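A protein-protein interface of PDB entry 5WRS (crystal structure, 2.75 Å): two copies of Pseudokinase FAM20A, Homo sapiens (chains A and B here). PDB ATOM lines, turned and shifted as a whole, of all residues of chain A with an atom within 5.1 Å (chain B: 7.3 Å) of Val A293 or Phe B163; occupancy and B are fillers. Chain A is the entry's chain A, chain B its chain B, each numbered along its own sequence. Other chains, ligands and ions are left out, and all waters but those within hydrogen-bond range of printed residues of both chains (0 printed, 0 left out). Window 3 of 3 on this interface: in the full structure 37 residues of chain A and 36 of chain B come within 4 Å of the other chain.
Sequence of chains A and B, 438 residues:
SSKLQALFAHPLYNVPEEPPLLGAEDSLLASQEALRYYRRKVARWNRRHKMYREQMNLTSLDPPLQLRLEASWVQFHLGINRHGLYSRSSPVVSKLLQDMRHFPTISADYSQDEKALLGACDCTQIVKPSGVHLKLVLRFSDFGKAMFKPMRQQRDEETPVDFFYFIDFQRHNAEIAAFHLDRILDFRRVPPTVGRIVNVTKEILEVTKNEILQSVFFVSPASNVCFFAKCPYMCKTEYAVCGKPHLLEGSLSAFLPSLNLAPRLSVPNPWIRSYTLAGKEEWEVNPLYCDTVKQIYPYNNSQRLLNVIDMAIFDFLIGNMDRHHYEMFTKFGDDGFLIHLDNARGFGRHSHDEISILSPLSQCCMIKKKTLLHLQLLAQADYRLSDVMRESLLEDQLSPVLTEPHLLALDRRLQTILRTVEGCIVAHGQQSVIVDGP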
ATOM      1  N   PRO A 268      18.544  26.105  -1.971  1.00  0.00           N
ATOM      2  CA  PRO A 268      18.185  25.337  -3.169  1.00  0.00           C
ATOM      3  C   PRO A 268      17.680  23.944  -2.822  1.00  0.00           C
ATOM      4  O   PRO A 268      18.167  23.296  -1.892  1.00  0.00           O
ATOM      5  CB  PRO A 268      19.499  25.274  -3.959  1.00  0.00           C
ATOM      6  CG  PRO A 268      20.568  25.509  -2.942  1.00  0.00           C
ATOM      7  CD  PRO A 268      19.974  26.455  -1.944  1.00  0.00           C
ATOM      8  N   PRO A 270      17.669  20.262  -3.511  1.00  0.00           N
ATOM      9  CA  PRO A 270      18.577  19.322  -4.192  1.00  0.00           C
ATOM     10  C   PRO A 270      17.883  18.363  -5.151  1.00  0.00           C
ATOM     11  O   PRO A 270      18.573  17.707  -5.941  1.00  0.00           O
ATOM     12  CB  PRO A 270      19.236  18.563  -3.031  1.00  0.00           C
ATOM     13  CG  PRO A 270      19.063  19.455  -1.842  1.00  0.00           C
ATOM     14  CD  PRO A 270      17.745  20.137  -2.047  1.00  0.00           C
ATOM     15  N   TRP A 271      16.554  18.257  -5.110  1.00  0.00           N
ATOM     16  CA  TRP A 271      15.812  17.366  -5.991  1.00  0.00           C
ATOM     17  C   TRP A 271      14.980  18.130  -7.016  1.00  0.00           C
ATOM     18  O   TRP A 271      14.027  17.574  -7.573  1.00  0.00           O
ATOM     19  CB  TRP A 271      14.913  16.437  -5.174  1.00  0.00           C
ATOM     20  CG  TRP A 271      15.647  15.353  -4.458  1.00  0.00           C
ATOM     21  CD1 TRP A 271      15.935  14.107  -4.931  1.00  0.00           C
ATOM     22  CD2 TRP A 271      16.191  15.416  -3.135  1.00  0.00           C
ATOM     23  NE1 TRP A 271      16.622  13.388  -3.984  1.00  0.00           N
ATOM     24  CE2 TRP A 271      16.793  14.169  -2.871  1.00  0.00           C
ATOM     25  CE3 TRP A 271      16.226  16.405  -2.146  1.00  0.00           C
ATOM     26  CZ2 TRP A 271      17.422  13.885  -1.661  1.00  0.00           C
ATOM     27  CZ3 TRP A 271      16.853  16.121  -0.946  1.00  0.00           C
ATOM     28  CH2 TRP A 271      17.441  14.871  -0.713  1.00  0.00           C
ATOM     29  N   TYR A 289      21.868   8.726  -4.936  1.00  0.00           N
ATOM     30  CA  TYR A 289      21.880  10.182  -4.821  1.00  0.00           C
ATOM     31  C   TYR A 289      21.596  10.631  -3.393  1.00  0.00           C
ATOM     32  O   TYR A 289      22.333  11.452  -2.832  1.00  0.00           O
ATOM     33  CB  TYR A 289      20.872  10.794  -5.791  1.00  0.00           C
ATOM     34  CG  TYR A 289      20.901  12.307  -5.829  1.00  0.00           C
ATOM     35  CD1 TYR A 289      22.032  12.988  -6.256  1.00  0.00           C
ATOM     36  CD2 TYR A 289      19.795  13.052  -5.443  1.00  0.00           C
ATOM     37  CE1 TYR A 289      22.061  14.372  -6.296  1.00  0.00           C
ATOM     38  CE2 TYR A 289      19.814  14.435  -5.484  1.00  0.00           C
ATOM     39  CZ  TYR A 289      20.949  15.088  -5.909  1.00  0.00           C
ATOM     40  OH  TYR A 289      20.968  16.465  -5.946  1.00  0.00           O
ATOM     41  N   CYS A 290      20.527  10.107  -2.782  1.00  0.00           N
ATOM     42  CA  CYS A 290      20.219  10.506  -1.412  1.00  0.00           C
ATOM     43  C   CYS A 290      21.258   9.990  -0.425  1.00  0.00           C
ATOM     44  O   CYS A 290      21.511  10.641   0.594  1.00  0.00           O
ATOM     45  CB  CYS A 290      18.819  10.040  -1.004  1.00  0.00           C
ATOM     46  SG  CYS A 290      18.362  10.636   0.652  1.00  0.00           S
ATOM     47  N   ASP A 291      21.864   8.830  -0.701  1.00  0.00           N
ATOM     48  CA  ASP A 291      22.976   8.371   0.129  1.00  0.00           C
ATOM     49  C   ASP A 291      24.099   9.399   0.169  1.00  0.00           C
ATOM     50  O   ASP A 291      24.788   9.528   1.188  1.00  0.00           O
ATOM     51  CB  ASP A 291      23.509   7.030  -0.381  1.00  0.00           C
ATOM     52  CG  ASP A 291      22.560   5.880  -0.106  1.00  0.00           C
ATOM     53  OD1 ASP A 291      21.849   5.925   0.921  1.00  0.00           O
ATOM     54  OD2 ASP A 291      22.535   4.926  -0.912  1.00  0.00           O
ATOM     55  N   THR A 292      24.297  10.138  -0.924  1.00  0.00           N
ATOM     56  CA  THR A 292      25.297  11.199  -0.947  1.00  0.00           C
ATOM     57  C   THR A 292      24.791  12.461  -0.257  1.00  0.00           C
ATOM     58  O   THR A 292      25.532  13.094   0.502  1.00  0.00           O
ATOM     59  CB  THR A 292      25.699  11.506  -2.389  1.00  0.00           C
ATOM     60  OG1 THR A 292      26.140  10.302  -3.029  1.00  0.00           O
ATOM     61  CG2 THR A 292      26.818  12.535  -2.425  1.00  0.00           C
ATOM     62  N   VAL A 293      23.537  12.844  -0.520  1.00  0.00           N
ATOM     63  CA  VAL A 293      22.964  14.031   0.112  1.00  0.00           C
ATOM     64  C   VAL A 293      22.912  13.863   1.628  1.00  0.00           C
ATOM     65  O   VAL A 293      23.116  14.824   2.381  1.00  0.00           O
ATOM     66  CB  VAL A 293      21.573  14.329  -0.478  1.00  0.00           C
ATOM     67  CG1 VAL A 293      20.945  15.533   0.207  1.00  0.00           C
ATOM     68  CG2 VAL A 293      21.671  14.558  -1.975  1.00  0.00           C
ATOM     69  N   LYS A 294      22.637  12.641   2.100  1.00  0.00           N
ATOM     70  CA  LYS A 294      22.619  12.380   3.538  1.00  0.00           C
ATOM     71  C   LYS A 294      23.949  12.721   4.200  1.00  0.00           C
ATOM     72  O   LYS A 294      23.986  12.997   5.403  1.00  0.00           O
ATOM     73  CB  LYS A 294      22.266  10.917   3.813  1.00  0.00           C
ATOM     74  CG  LYS A 294      20.790  10.575   3.698  1.00  0.00           C
ATOM     75  CD  LYS A 294      20.567   9.080   3.890  1.00  0.00           C
ATOM     76  CE  LYS A 294      19.131   8.679   3.581  1.00  0.00           C
ATOM     77  NZ  LYS A 294      18.788   7.345   4.150  1.00  0.00           N
ATOM     78  N   GLN A 295      25.044  12.699   3.444  1.00  0.00           N
ATOM     79  CA  GLN A 295      26.366  13.003   3.973  1.00  0.00           C
ATOM     80  C   GLN A 295      26.776  14.450   3.735  1.00  0.00           C
ATOM     81  O   GLN A 295      27.940  14.798   3.954  1.00  0.00           O
ATOM     82  CB  GLN A 295      27.407  12.062   3.362  1.00  0.00           C
ATOM     83  CG  GLN A 295      27.119  10.586   3.578  1.00  0.00           C
ATOM     84  CD  GLN A 295      28.174   9.694   2.951  1.00  0.00           C
ATOM     85  OE1 GLN A 295      29.128   9.282   3.611  1.00  0.00           O
ATOM     86  NE2 GLN A 295      28.009   9.396   1.667  1.00  0.00           N
ATOM     87  N   ILE A 296      25.852  15.297   3.292  1.00  0.00           N
ATOM     88  CA  ILE A 296      26.140  16.689   2.966  1.00  0.00           C
ATOM     89  C   ILE A 296      25.335  17.580   3.902  1.00  0.00           C
ATOM     90  O   ILE A 296      24.102  17.485   3.950  1.00  0.00           O
ATOM     91  CB  ILE A 296      25.821  17.008   1.497  1.00  0.00           C
ATOM     92  CG1 ILE A 296      26.745  16.214   0.571  1.00  0.00           C
ATOM     93  CG2 ILE A 296      25.947  18.500   1.236  1.00  0.00           C
ATOM     94  CD1 ILE A 296      26.526  16.497  -0.899  1.00  0.00           C
ATOM     95  N   TYR A 299      21.880  18.246   5.441  1.00  0.00           N
ATOM     96  CA  TYR A 299      21.024  17.072   5.338  1.00  0.00           C
ATOM     97  C   TYR A 299      21.564  15.866   6.097  1.00  0.00           C
ATOM     98  O   TYR A 299      20.998  14.773   5.972  1.00  0.00           O
ATOM     99  CB  TYR A 299      20.808  16.724   3.865  1.00  0.00           C
ATOM    100  CG  TYR A 299      20.264  17.892   3.080  1.00  0.00           C
ATOM    101  CD1 TYR A 299      18.918  18.229   3.145  1.00  0.00           C
ATOM    102  CD2 TYR A 299      21.098  18.675   2.295  1.00  0.00           C
ATOM    103  CE1 TYR A 299      18.417  19.303   2.438  1.00  0.00           C
ATOM    104  CE2 TYR A 299      20.605  19.750   1.583  1.00  0.00           C
ATOM    105  CZ  TYR A 299      19.264  20.060   1.660  1.00  0.00           C
ATOM    106  OH  TYR A 299      18.768  21.130   0.955  1.00  0.00           O
ATOM    107  N   ASN A 300      22.628  16.032   6.884  1.00  0.00           N
ATOM    108  CA  ASN A 300      23.117  14.927   7.699  1.00  0.00           C
ATOM    109  C   ASN A 300      22.268  14.714   8.946  1.00  0.00           C
ATOM    110  O   ASN A 300      22.215  13.594   9.466  1.00  0.00           O
ATOM    111  CB  ASN A 300      24.584  15.150   8.074  1.00  0.00           C
ATOM    112  CG  ASN A 300      24.831  16.510   8.683  1.00  0.00           C
ATOM    113  OD1 ASN A 300      24.415  17.532   8.140  1.00  0.00           O
ATOM    114  ND2 ASN A 300      25.516  16.531   9.819  1.00  0.00           N
ATOM    115  N   LEU A 305      16.171  16.603   6.460  1.00  0.00           N
ATOM    116  CA  LEU A 305      15.808  15.733   5.346  1.00  0.00           C
ATOM    117  C   LEU A 305      14.337  15.333   5.413  1.00  0.00           C
ATOM    118  O   LEU A 305      13.664  15.255   4.379  1.00  0.00           O
ATOM    119  CB  LEU A 305      16.709  14.498   5.333  1.00  0.00           C
ATOM    120  CG  LEU A 305      16.618  13.585   4.108  1.00  0.00           C
ATOM    121  CD1 LEU A 305      16.875  14.378   2.840  1.00  0.00           C
ATOM    122  CD2 LEU A 305      17.605  12.433   4.223  1.00  0.00           C
ATOM    123  N   ASP B 156      32.401  25.212  -0.711  1.00  0.00           N
ATOM    124  CA  ASP B 156      31.042  25.240  -0.177  1.00  0.00           C
ATOM    125  C   ASP B 156      30.990  25.364   1.341  1.00  0.00           C
ATOM    126  O   ASP B 156      29.919  25.663   1.878  1.00  0.00           O
ATOM    127  CB  ASP B 156      30.262  23.998  -0.618  1.00  0.00           C
ATOM    128  CG  ASP B 156      30.981  22.706  -0.294  1.00  0.00           C
ATOM    129  OD1 ASP B 156      32.162  22.571  -0.675  1.00  0.00           O
ATOM    130  OD2 ASP B 156      30.364  21.825   0.340  1.00  0.00           O
ATOM    131  N   THR B 159      30.172  28.834   1.889  1.00  0.00           N
ATOM    132  CA  THR B 159      28.847  29.176   1.373  1.00  0.00           C
ATOM    133  C   THR B 159      27.879  28.114   1.872  1.00  0.00           C
ATOM    134  O   THR B 159      27.491  27.206   1.123  1.00  0.00           O
ATOM    135  CB  THR B 159      28.848  29.258  -0.154  1.00  0.00           C
ATOM    136  OG1 THR B 159      29.128  27.963  -0.699  1.00  0.00           O
ATOM    137  CG2 THR B 159      29.909  30.235  -0.629  1.00  0.00           C
ATOM    138  N   PRO B 160      27.469  28.196   3.141  1.00  0.00           N
ATOM    139  CA  PRO B 160      26.680  27.101   3.732  1.00  0.00           C
ATOM    140  C   PRO B 160      25.352  26.849   3.039  1.00  0.00           C
ATOM    141  O   PRO B 160      24.851  25.719   3.083  1.00  0.00           O
ATOM    142  CB  PRO B 160      26.484  27.559   5.184  1.00  0.00           C
ATOM    143  CG  PRO B 160      26.669  29.040   5.150  1.00  0.00           C
ATOM    144  CD  PRO B 160      27.698  29.295   4.094  1.00  0.00           C
ATOM    145  N   VAL B 161      24.764  27.863   2.403  1.00  0.00           N
ATOM    146  CA  VAL B 161      23.458  27.681   1.777  1.00  0.00           C
ATOM    147  C   VAL B 161      23.567  27.016   0.408  1.00  0.00           C
ATOM    148  O   VAL B 161      22.608  26.372  -0.038  1.00  0.00           O
ATOM    149  CB  VAL B 161      22.723  29.032   1.699  1.00  0.00           C
ATOM    150  CG1 VAL B 161      22.489  29.463   0.256  1.00  0.00           C
ATOM    151  CG2 VAL B 161      21.410  28.966   2.466  1.00  0.00           C
ATOM    152  N   ASP B 162      24.714  27.132  -0.258  1.00  0.00           N
ATOM    153  CA  ASP B 162      24.872  26.568  -1.592  1.00  0.00           C
ATOM    154  C   ASP B 162      24.953  25.047  -1.537  1.00  0.00           C
ATOM    155  O   ASP B 162      25.634  24.473  -0.683  1.00  0.00           O
ATOM    156  CB  ASP B 162      26.125  27.132  -2.262  1.00  0.00           C
ATOM    157  CG  ASP B 162      25.970  28.586  -2.656  1.00  0.00           C
ATOM    158  OD1 ASP B 162      24.923  29.185  -2.329  1.00  0.00           O
ATOM    159  OD2 ASP B 162      26.898  29.135  -3.288  1.00  0.00           O
ATOM    160  N   PHE B 163      24.255  24.396  -2.464  1.00  0.00           N
ATOM    161  CA  PHE B 163      24.305  22.946  -2.596  1.00  0.00           C
ATOM    162  C   PHE B 163      25.476  22.568  -3.493  1.00  0.00           C
ATOM    163  O   PHE B 163      25.630  23.124  -4.586  1.00  0.00           O
ATOM    164  CB  PHE B 163      22.989  22.406  -3.158  1.00  0.00           C
ATOM    165  CG  PHE B 163      22.929  20.907  -3.224  1.00  0.00           C
ATOM    166  CD1 PHE B 163      23.042  20.145  -2.071  1.00  0.00           C
ATOM    167  CD2 PHE B 163      22.734  20.260  -4.434  1.00  0.00           C
ATOM    168  CE1 PHE B 163      22.986  18.766  -2.126  1.00  0.00           C
ATOM    169  CE2 PHE B 163      22.672  18.879  -4.494  1.00  0.00           C
ATOM    170  CZ  PHE B 163      22.799  18.131  -3.338  1.00  0.00           C
ATOM    171  N   PHE B 164      26.300  21.628  -3.017  1.00  0.00           N
ATOM    172  CA  PHE B 164      27.590  21.342  -3.643  1.00  0.00           C
ATOM    173  C   PHE B 164      27.464  21.082  -5.141  1.00  0.00           C
ATOM    174  O   PHE B 164      28.173  21.694  -5.949  1.00  0.00           O
ATOM    175  CB  PHE B 164      28.249  20.147  -2.952  1.00  0.00           C
ATOM    176  CG  PHE B 164      29.569  19.756  -3.550  1.00  0.00           C
ATOM    177  CD1 PHE B 164      30.715  20.484  -3.270  1.00  0.00           C
ATOM    178  CD2 PHE B 164      29.666  18.659  -4.392  1.00  0.00           C
ATOM    179  CE1 PHE B 164      31.933  20.126  -3.824  1.00  0.00           C
ATOM    180  CE2 PHE B 164      30.880  18.298  -4.947  1.00  0.00           C
ATOM    181  CZ  PHE B 164      32.014  19.031  -4.661  1.00  0.00           C
ATOM    182  N   TYR B 165      26.573  20.175  -5.532  1.00  0.00           N
ATOM    183  CA  TYR B 165      26.472  19.757  -6.925  1.00  0.00           C
ATOM    184  C   TYR B 165      25.766  20.776  -7.813  1.00  0.00           C
ATOM    185  O   TYR B 165      25.501  20.473  -8.982  1.00  0.00           O
ATOM    186  CB  TYR B 165      25.771  18.400  -7.014  1.00  0.00           C
ATOM    187  CG  TYR B 165      26.544  17.296  -6.328  1.00  0.00           C
ATOM    188  CD1 TYR B 165      27.639  16.705  -6.942  1.00  0.00           C
ATOM    189  CD2 TYR B 165      26.188  16.857  -5.059  1.00  0.00           C
ATOM    190  CE1 TYR B 165      28.355  15.702  -6.316  1.00  0.00           C
ATOM    191  CE2 TYR B 165      26.899  15.852  -4.426  1.00  0.00           C
ATOM    192  CZ  TYR B 165      27.980  15.280  -5.060  1.00  0.00           C
ATOM    193  OH  TYR B 165      28.691  14.281  -4.435  1.00  0.00           O
ATOM    194  N   PHE B 166      25.460  21.967  -7.300  1.00  0.00           N
ATOM    195  CA  PHE B 166      24.908  23.046  -8.108  1.00  0.00           C
ATOM    196  C   PHE B 166      25.871  24.214  -8.261  1.00  0.00           C
ATOM    197  O   PHE B 166      25.542  25.185  -8.951  1.00  0.00           O
ATOM    198  CB  PHE B 166      23.589  23.550  -7.507  1.00  0.00           C
ATOM    199  CG  PHE B 166      22.459  22.559  -7.586  1.00  0.00           C
ATOM    200  CD1 PHE B 166      22.558  21.426  -8.375  1.00  0.00           C
ATOM    201  CD2 PHE B 166      21.292  22.768  -6.868  1.00  0.00           C
ATOM    202  CE1 PHE B 166      21.519  20.517  -8.444  1.00  0.00           C
ATOM    203  CE2 PHE B 166      20.250  21.864  -6.934  1.00  0.00           C
ATOM    204  CZ  PHE B 166      20.363  20.737  -7.722  1.00  0.00           C
ATOM    205  N   ILE B 167      27.046  24.145  -7.643  1.00  0.00           N
ATOM    206  CA  ILE B 167      27.989  25.257  -7.647  1.00  0.00           C
ATOM    207  C   ILE B 167      28.688  25.318  -8.999  1.00  0.00           C
ATOM    208  O   ILE B 167      29.133  24.293  -9.531  1.00  0.00           O
ATOM    209  CB  ILE B 167      28.999  25.110  -6.499  1.00  0.00           C
ATOM    210  CG1 ILE B 167      28.273  25.167  -5.153  1.00  0.00           C
ATOM    211  CG2 ILE B 167      30.072  26.184  -6.587  1.00  0.00           C
ATOM    212  CD1 ILE B 167      29.167  24.939  -3.958  1.00  0.00           C
ATOM    213  N   ASP B 168      28.788  26.527  -9.554  1.00  0.00           N
ATOM    214  CA  ASP B 168      29.393  26.762 -10.867  1.00  0.00           C
ATOM    215  C   ASP B 168      30.916  26.860 -10.732  1.00  0.00           C
ATOM    216  O   ASP B 168      31.531  27.915 -10.896  1.00  0.00           O
ATOM    217  CB  ASP B 168      28.798  28.015 -11.495  1.00  0.00           C
ATOM    218  CG  ASP B 168      28.845  29.217 -10.563  1.00  0.00           C
ATOM    219  OD1 ASP B 168      29.227  29.045  -9.385  1.00  0.00           O
ATOM    220  OD2 ASP B 168      28.492  30.332 -11.004  1.00  0.00           O
ATOM    221  N   PHE B 169      31.531  25.719 -10.406  1.00  0.00           N
ATOM    222  CA  PHE B 169      32.984  25.689 -10.266  1.00  0.00           C
ATOM    223  C   PHE B 169      33.675  25.940 -11.601  1.00  0.00           C
ATOM    224  O   PHE B 169      34.682  26.655 -11.662  1.00  0.00           O
ATOM    225  CB  PHE B 169      33.423  24.353  -9.663  1.00  0.00           C
ATOM    226  CG  PHE B 169      33.223  24.267  -8.178  1.00  0.00           C
ATOM    227  CD1 PHE B 169      33.857  25.158  -7.326  1.00  0.00           C
ATOM    228  CD2 PHE B 169      32.382  23.309  -7.634  1.00  0.00           C
ATOM    229  CE1 PHE B 169      33.664  25.083  -5.954  1.00  0.00           C
ATOM    230  CE2 PHE B 169      32.184  23.230  -6.267  1.00  0.00           C
ATOM    231  CZ  PHE B 169      32.825  24.118  -5.426  1.00  0.00           C
ATOM    232  N   ARG B 349      30.028  18.489 -15.509  1.00  0.00           N
ATOM    233  CA  ARG B 349      30.125  17.058 -15.240  1.00  0.00           C
ATOM    234  C   ARG B 349      30.655  16.378 -16.493  1.00  0.00           C
ATOM    235  O   ARG B 349      29.929  16.245 -17.482  1.00  0.00           O
ATOM    236  CB  ARG B 349      28.777  16.458 -14.833  1.00  0.00           C
ATOM    237  CG  ARG B 349      28.243  16.920 -13.489  1.00  0.00           C
ATOM    238  CD  ARG B 349      27.002  16.123 -13.115  1.00  0.00           C
ATOM    239  NE  ARG B 349      26.235  16.741 -12.039  1.00  0.00           N
ATOM    240  CZ  ARG B 349      25.239  17.599 -12.233  1.00  0.00           C
ATOM    241  NH1 ARG B 349      24.889  17.944 -13.466  1.00  0.00           N
ATOM    242  NH2 ARG B 349      24.590  18.112 -11.196  1.00  0.00           N
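Of the printed residues of chain B, Pro A268 touches Val B161 (3.3 Å) and Phe B163 (3.9 Å).
Of the printed residues of chain B, Val A293 touches Phe B163 (3.99 Å).
Of the printed residues of chain B, Ile A296 touches Tyr B165.
Asn A300 touches none of the printed residues of chain B.
Leu A305 touches none of the printed residues of chain B.
Of the printed residues of chain A, Phe B163 touches Pro A268 (3.9 Å), Pro A270 (3.6 Å), Tyr A289 (3.3 Å) and Val A293 (3.99 Å).
Of the printed residues of chain A, Tyr B165 touches Thr A292 and Ile A296.
The nearest printed residue of chain B that does not touch Val A293 is Tyr B165 (5.9 Å).
CD of Pro A268 touches O of Val B161, at 3.3 Å.
Phe B163 touches Pro A268.
Phe B163 touches Pro A270.
Pro A270 touches Phe B166 (O to CZ, 3.9 Å).
Phe B163 touches Tyr A289 (CE2 to OH, 3.3 Å).
CG2 of Thr A292 touches OH of Tyr B165, 3.3 Å away.
Phe B163 touches Val A293 (CZ to CG2, 3.99 Å).
Ile A296 touches Tyr B165 (CD1 to CE2, 3.6 Å).
Of the 13 printed residues of chain B, 4 touch a printed residue of chain A.
Printed residues of chain B that touch a printed residue of chain A: Val B161, Phe B163, Tyr B165 and Phe B166.
Hydrophobic or aromatic side chains of chain A that line the printed part of chain B: Pro A268, Pro A270, Tyr A289, Val A293 and Ile A296.
Among the printed residues, 8 pairs touch across the chains.
Among the printed residues, no Asp or Glu carboxylate lies within 4 Å of a Lys or Arg side-chain nitrogen of the other chain.
No position is printed for both chains.
The guanidinium group (NH2) of Arg B349 lies within hydrogen-bond range of the backbone carbonyl oxygen (O) of Tyr B165 (3.4 Å).
The backbone carbonyl oxygen (O) of Pro A270 lies within hydrogen-bond range of the side-chain hydroxyl (OH) of Tyr A289 (2.7 Å).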
